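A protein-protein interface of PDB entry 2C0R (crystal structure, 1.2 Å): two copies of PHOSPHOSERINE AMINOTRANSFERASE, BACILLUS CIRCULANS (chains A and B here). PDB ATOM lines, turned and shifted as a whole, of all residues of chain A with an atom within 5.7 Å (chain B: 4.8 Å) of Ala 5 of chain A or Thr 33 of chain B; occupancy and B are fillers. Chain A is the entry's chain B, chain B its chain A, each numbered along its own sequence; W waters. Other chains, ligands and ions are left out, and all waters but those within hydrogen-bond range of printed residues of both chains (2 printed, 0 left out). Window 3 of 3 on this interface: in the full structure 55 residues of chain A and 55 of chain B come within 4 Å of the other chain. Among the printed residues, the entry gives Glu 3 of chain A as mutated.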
ATOM      1  N   GLU A   3      -7.373   1.961   2.563  1.00  0.00           N
ATOM      2  CA  GLU A   3      -8.049   2.848   3.486  1.00  0.00           C
ATOM      3  C   GLU A   3      -8.749   1.998   4.553  1.00  0.00           C
ATOM      4  O   GLU A   3      -9.370   2.575   5.444  1.00  0.00           O
ATOM      5  CB  GLU A   3      -9.037   3.750   2.757  1.00  0.00           C
ATOM      6  CG  GLU A   3      -8.992   5.209   3.145  1.00  0.00           C
ATOM      7  CD  GLU A   3      -8.031   6.058   2.345  1.00  0.00           C
ATOM      8  OE1 GLU A   3      -6.808   5.996   2.603  1.00  0.00           O
ATOM      9  OE2 GLU A   3      -8.461   6.813   1.442  1.00  0.00           O
ATOM     10  N   ARG A   4      -8.664   0.683   4.488  1.00  0.00           N
ATOM     11  CA  ARG A   4      -9.270  -0.197   5.490  1.00  0.00           C
ATOM     12  C   ARG A   4      -8.624   0.037   6.844  1.00  0.00           C
ATOM     13  O   ARG A   4      -7.390  -0.004   6.963  1.00  0.00           O
ATOM     14  CB  ARG A   4      -9.154  -1.656   5.070  1.00  0.00           C
ATOM     15  CG  ARG A   4     -10.039  -1.950   3.842  1.00  0.00           C
ATOM     16  CD  ARG A   4     -11.479  -2.188   4.248  1.00  0.00           C
ATOM     17  NE  ARG A   4     -11.607  -3.546   4.812  1.00  0.00           N
ATOM     18  CZ  ARG A   4     -12.666  -3.912   5.537  1.00  0.00           C
ATOM     19  NH1 ARG A   4     -13.677  -3.071   5.788  1.00  0.00           N
ATOM     20  NH2 ARG A   4     -12.706  -5.150   5.988  1.00  0.00           N
ATOM     21  N   ALA A   5      -9.452   0.206   7.878  1.00  0.00           N
ATOM     22  CA  ALA A   5      -8.915   0.306   9.232  1.00  0.00           C
ATOM     23  C   ALA A   5      -8.198  -0.988   9.631  1.00  0.00           C
ATOM     24  O   ALA A   5      -8.577  -2.062   9.152  1.00  0.00           O
ATOM     25  CB  ALA A   5     -10.044   0.541  10.224  1.00  0.00           C
ATOM     26  N   TYR A   6      -7.212  -0.884  10.508  1.00  0.00           N
ATOM     27  CA  TYR A   6      -6.603  -2.074  11.127  1.00  0.00           C
ATOM     28  C   TYR A   6      -7.517  -2.452  12.282  1.00  0.00           C
ATOM     29  O   TYR A   6      -7.374  -1.974  13.405  1.00  0.00           O
ATOM     30  CB  TYR A   6      -5.204  -1.765  11.578  1.00  0.00           C
ATOM     31  CG  TYR A   6      -4.236  -1.275  10.530  1.00  0.00           C
ATOM     32  CD1 TYR A   6      -3.463  -0.158  10.796  1.00  0.00           C
ATOM     33  CD2 TYR A   6      -4.098  -1.936   9.326  1.00  0.00           C
ATOM     34  CE1 TYR A   6      -2.563   0.280   9.812  1.00  0.00           C
ATOM     35  CE2 TYR A   6      -3.216  -1.527   8.344  1.00  0.00           C
ATOM     36  CZ  TYR A   6      -2.441  -0.392   8.621  1.00  0.00           C
ATOM     37  OH  TYR A   6      -1.557   0.037   7.646  1.00  0.00           O
ATOM     38  N   ASN A   7      -8.472  -3.308  11.911  1.00  0.00           N
ATOM     39  CA  ASN A   7      -9.583  -3.607  12.773  1.00  0.00           C
ATOM     40  C   ASN A   7      -9.296  -4.853  13.638  1.00  0.00           C
ATOM     41  O   ASN A   7      -9.317  -5.970  13.132  1.00  0.00           O
ATOM     42  CB  ASN A   7     -10.824  -3.875  11.900  1.00  0.00           C
ATOM     43  CG  ASN A   7     -12.078  -4.054  12.742  1.00  0.00           C
ATOM     44  OD1 ASN A   7     -12.032  -3.925  13.983  1.00  0.00           O
ATOM     45  ND2 ASN A   7     -13.209  -4.348  12.112  1.00  0.00           N
ATOM     46  N   GLY A 321      -4.758   4.255  12.694  1.00  0.00           N
ATOM     47  CA  GLY A 321      -5.763   3.426  12.012  1.00  0.00           C
ATOM     48  C   GLY A 321      -6.139   2.154  12.698  1.00  0.00           C
ATOM     49  O   GLY A 321      -6.941   1.387  12.140  1.00  0.00           O
ATOM     50  N   VAL A 323      -8.171  -0.023  15.515  1.00  0.00           N
ATOM     51  CA  VAL A 323      -9.370   0.049  16.351  1.00  0.00           C
ATOM     52  C   VAL A 323      -9.442  -1.238  17.177  1.00  0.00           C
ATOM     53  O   VAL A 323      -9.081  -2.303  16.683  1.00  0.00           O
ATOM     54  CB  VAL A 323     -10.630   0.270  15.505  1.00  0.00           C
ATOM     55  CG1 VAL A 323     -10.644  -0.642  14.293  1.00  0.00           C
ATOM     56  CG2 VAL A 323     -11.899   0.045  16.313  1.00  0.00           C
ATOM     57  N   SER A 346      -2.863  -6.411   8.727  1.00  0.00           N
ATOM     58  CA  SER A 346      -3.176  -5.728   9.973  1.00  0.00           C
ATOM     59  C   SER A 346      -2.218  -6.089  11.113  1.00  0.00           C
ATOM     60  O   SER A 346      -1.829  -5.245  11.909  1.00  0.00           O
ATOM     61  CB  SER A 346      -4.603  -5.999  10.441  1.00  0.00           C
ATOM     62  OG  SER A 346      -5.509  -5.333   9.578  1.00  0.00           O
ATOM     63  N   ASP B  29     -17.567   0.880   3.345  1.00  0.00           N
ATOM     64  CA  ASP B  29     -16.879   1.893   4.133  1.00  0.00           C
ATOM     65  C   ASP B  29     -17.891   2.903   4.663  1.00  0.00           C
ATOM     66  O   ASP B  29     -18.376   3.712   3.874  1.00  0.00           O
ATOM     67  CB  ASP B  29     -15.842   2.584   3.263  1.00  0.00           C
ATOM     68  CG  ASP B  29     -14.922   3.500   4.074  1.00  0.00           C
ATOM     69  OD1 ASP B  29     -15.152   3.787   5.266  1.00  0.00           O
ATOM     70  OD2 ASP B  29     -13.917   3.967   3.491  1.00  0.00           O
ATOM     71  N   TYR B  30     -18.180   2.798   5.953  1.00  0.00           N
ATOM     72  CA  TYR B  30     -19.153   3.688   6.572  1.00  0.00           C
ATOM     73  C   TYR B  30     -18.446   4.964   7.004  1.00  0.00           C
ATOM     74  O   TYR B  30     -17.560   4.905   7.849  1.00  0.00           O
ATOM     75  CB  TYR B  30     -19.797   3.027   7.753  1.00  0.00           C
ATOM     76  CG  TYR B  30     -20.730   3.839   8.586  1.00  0.00           C
ATOM     77  CD1 TYR B  30     -22.100   3.790   8.272  1.00  0.00           C
ATOM     78  CD2 TYR B  30     -20.306   4.587   9.670  1.00  0.00           C
ATOM     79  CE1 TYR B  30     -23.025   4.522   9.024  1.00  0.00           C
ATOM     80  CE2 TYR B  30     -21.235   5.305  10.423  1.00  0.00           C
ATOM     81  CZ  TYR B  30     -22.573   5.262  10.100  1.00  0.00           C
ATOM     82  OH  TYR B  30     -23.411   5.992  10.901  1.00  0.00           O
ATOM     83  N   GLN B  31     -18.849   6.079   6.421  1.00  0.00           N
ATOM     84  CA  GLN B  31     -18.340   7.407   6.772  1.00  0.00           C
ATOM     85  C   GLN B  31     -16.824   7.522   6.920  1.00  0.00           C
ATOM     86  O   GLN B  31     -16.255   8.098   7.854  1.00  0.00           O
ATOM     87  CB  GLN B  31     -19.013   7.875   8.075  1.00  0.00           C
ATOM     88  CG  GLN B  31     -20.521   8.025   7.970  1.00  0.00           C
ATOM     89  CD  GLN B  31     -21.182   8.586   9.218  1.00  0.00           C
ATOM     90  OE1 GLN B  31     -20.581   9.016  10.206  1.00  0.00           O
ATOM     91  NE2 GLN B  31     -22.498   8.604   9.213  1.00  0.00           N
ATOM     92  N   HIS B  32     -16.104   6.975   5.943  1.00  0.00           N
ATOM     93  CA  HIS B  32     -14.664   7.055   5.850  1.00  0.00           C
ATOM     94  C   HIS B  32     -13.969   6.494   7.085  1.00  0.00           C
ATOM     95  O   HIS B  32     -12.860   6.885   7.375  1.00  0.00           O
ATOM     96  CB  HIS B  32     -14.156   8.500   5.537  1.00  0.00           C
ATOM     97  CG  HIS B  32     -14.688   8.900   4.184  1.00  0.00           C
ATOM     98  ND1 HIS B  32     -14.105   8.434   3.035  1.00  0.00           N
ATOM     99  CD2 HIS B  32     -15.749   9.646   3.815  1.00  0.00           C
ATOM    100  CE1 HIS B  32     -14.786   8.902   1.992  1.00  0.00           C
ATOM    101  NE2 HIS B  32     -15.784   9.646   2.442  1.00  0.00           N
ATOM    102  N   THR B  33     -14.593   5.555   7.773  1.00  0.00           N
ATOM    103  CA  THR B  33     -13.931   4.934   8.899  1.00  0.00           C
ATOM    104  C   THR B  33     -13.080   3.738   8.496  1.00  0.00           C
ATOM    105  O   THR B  33     -12.278   3.254   9.334  1.00  0.00           O
ATOM    106  CB  THR B  33     -14.941   4.374   9.916  1.00  0.00           C
ATOM    107  OG1 THR B  33     -15.723   3.402   9.221  1.00  0.00           O
ATOM    108  CG2 THR B  33     -15.833   5.475  10.478  1.00  0.00           C
ATOM    109  N   GLY B  34     -13.260   3.303   7.270  1.00  0.00           N
ATOM    110  CA  GLY B  34     -12.477   2.171   6.793  1.00  0.00           C
ATOM    111  C   GLY B  34     -13.014   0.868   7.369  1.00  0.00           C
ATOM    112  O   GLY B  34     -12.267  -0.131   7.401  1.00  0.00           O
ATOM    113  N   MET B  35     -14.271   0.886   7.809  1.00  0.00           N
ATOM    114  CA  MET B  35     -14.988  -0.293   8.256  1.00  0.00           C
ATOM    115  C   MET B  35     -16.443  -0.177   7.763  1.00  0.00           C
ATOM    116  O   MET B  35     -16.946   0.918   7.570  1.00  0.00           O
ATOM    117  CB  MET B  35     -14.987  -0.367   9.787  1.00  0.00           C
ATOM    118  CG  MET B  35     -13.651  -0.740  10.394  1.00  0.00           C
ATOM    119  SD  MET B  35     -13.758  -0.743  12.213  1.00  0.00           S
ATOM    120  CE  MET B  35     -13.791   1.010  12.508  1.00  0.00           C
ATOM    121  N   MET B  40     -18.092  -2.955  13.311  1.00  0.00           N
ATOM    122  CA  MET B  40     -17.684  -2.034  14.385  1.00  0.00           C
ATOM    123  C   MET B  40     -18.193  -2.542  15.725  1.00  0.00           C
ATOM    124  O   MET B  40     -19.171  -3.315  15.813  1.00  0.00           O
ATOM    125  CB  MET B  40     -18.339  -0.687  14.133  1.00  0.00           C
ATOM    126  CG  MET B  40     -17.834  -0.067  12.837  1.00  0.00           C
ATOM    127  SD  MET B  40     -18.549   1.577  12.801  1.00  0.00           S
ATOM    128  CE  MET B  40     -17.990   2.073  11.167  1.00  0.00           C
HETATM  129  O   HOH W   1     -14.047  -0.370   4.812  1.00  0.00           O
HETATM  130  O   HOH W   2     -11.236  -2.553   8.236  1.00  0.00           O
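No position is printed for both chains.
O of Glu 3 of chain A touches CA of Gly 34 of chain B, at 3.4 Å. Arg 4 of chain A touches Gly 34 of chain B (CA to O, 3.6 Å). Arg 4 of chain A touches Met 35 of chain B (NH1 to CA, 3.9 Å). Ala 5 of chain A touches Thr 33 of chain B (CB to O, 3.6 Å). CB of Ala 5 of chain A touches CG of Met 35 of chain B, 3.8 Å away. Val 323 of chain A touches Met 35 of chain B (CG1 to SD, 3.7 Å).
Water W2 lies within hydrogen-bond range of the backbone carbonyl oxygen of Gly 34 of chain B (2.8 Å), the backbone carbonyl oxygen of Ala 5 of chain A (2.9 Å) and the guanidinium group of Arg 4 of chain A (3.5 Å). Water W1 lies within hydrogen-bond range of NH1 of Arg 4 of chain A, O of Gly 34 of chain B and N of Met 35 of chain B.
The backbone carbonyl oxygen of Gly 34 of chain B lies within hydrogen-bond range of the backbone NH of Ala 5 of chain A, at 2.9 Å. The side-chain amide nitrogen of Asn 7 of chain A sits at hydrogen-bond distance from the side-chain sulfur of Met 35 of chain B (3.6 Å).
Thr 33 of chain B touches just one residue of chain A: Ala 5. Of the printed residues of chain A, Gly 34 of chain B touches Glu 3, Arg 4 and Ala 5. Printed residues of chain A within 4 Å of Met 35 of chain B: Arg 4, Ala 5, Asn 7 and Val 323. Printed residues of chain B within 4 Å of Glu 3 of chain A: Gly 34. Of the printed residues of chain B, Arg 4 of chain A touches Gly 34 (3.6 Å) and Met 35 (3.9 Å). Of the printed residues of chain B, Val 323 of chain A touches Met 35. His 32 of chain B touches none of the printed residues of chain A. Gln 31 of chain B touches none of the printed residues of chain A. The nearest printed residue of chain B that does not touch Ala 5 of chain A is Asp 29 of chain B (7.2 Å). The nearest residue of chain A that does not touch Thr 33 of chain B is Glu 3 of chain A (4.9 Å). The nearest printed residue of chain B that does not touch Val 323 of chain A is Met 40 of chain B (6.4 Å).
The backbone NH (N) of Thr 33 of chain B lies within hydrogen-bond range of the side-chain carboxylate (OD1) of Asp 29 of chain B (3.1 Å). The side-chain carboxylate (OD1) of Asp 29 of chain B is in hydrogen-bond range of the backbone NH (N) of Gly 34 of chain B, 2.8 Å away. The backbone carbonyl oxygen (O) of Tyr 30 of chain B is in hydrogen-bond range of the side-chain hydroxyl (OG1) of Thr 33 of chain B (2.7 Å). The backbone carbonyl oxygen (O) of Met 35 of chain B is in hydrogen-bond range of the backbone NH (N) of Tyr 30 of chain B (2.8 Å). OG1 of Thr 33 of chain B lies within hydrogen-bond range of O of Met 35 of chain B (3.2 Å). O of Tyr 6 of chain A sits at hydrogen-bond distance from N of Val 323 of chain A (3.0 Å).
Hydrophobic or aromatic side chains of chain A within 4 Å of the printed part of chain B: Ala 5 and Val 323. Hydrophobic or aromatic side chains of chain B within 4 Å of the printed part of chain A: Met 35. Along chain B the printed residues that touch a printed residue of chain A span positions 33 to 35. Among the printed residues, 8 pairs touch across the chains. Among the printed residues, no Asp or Glu carboxylate lies within 4 Å of a Lys or Arg side-chain nitrogen of the other chain.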
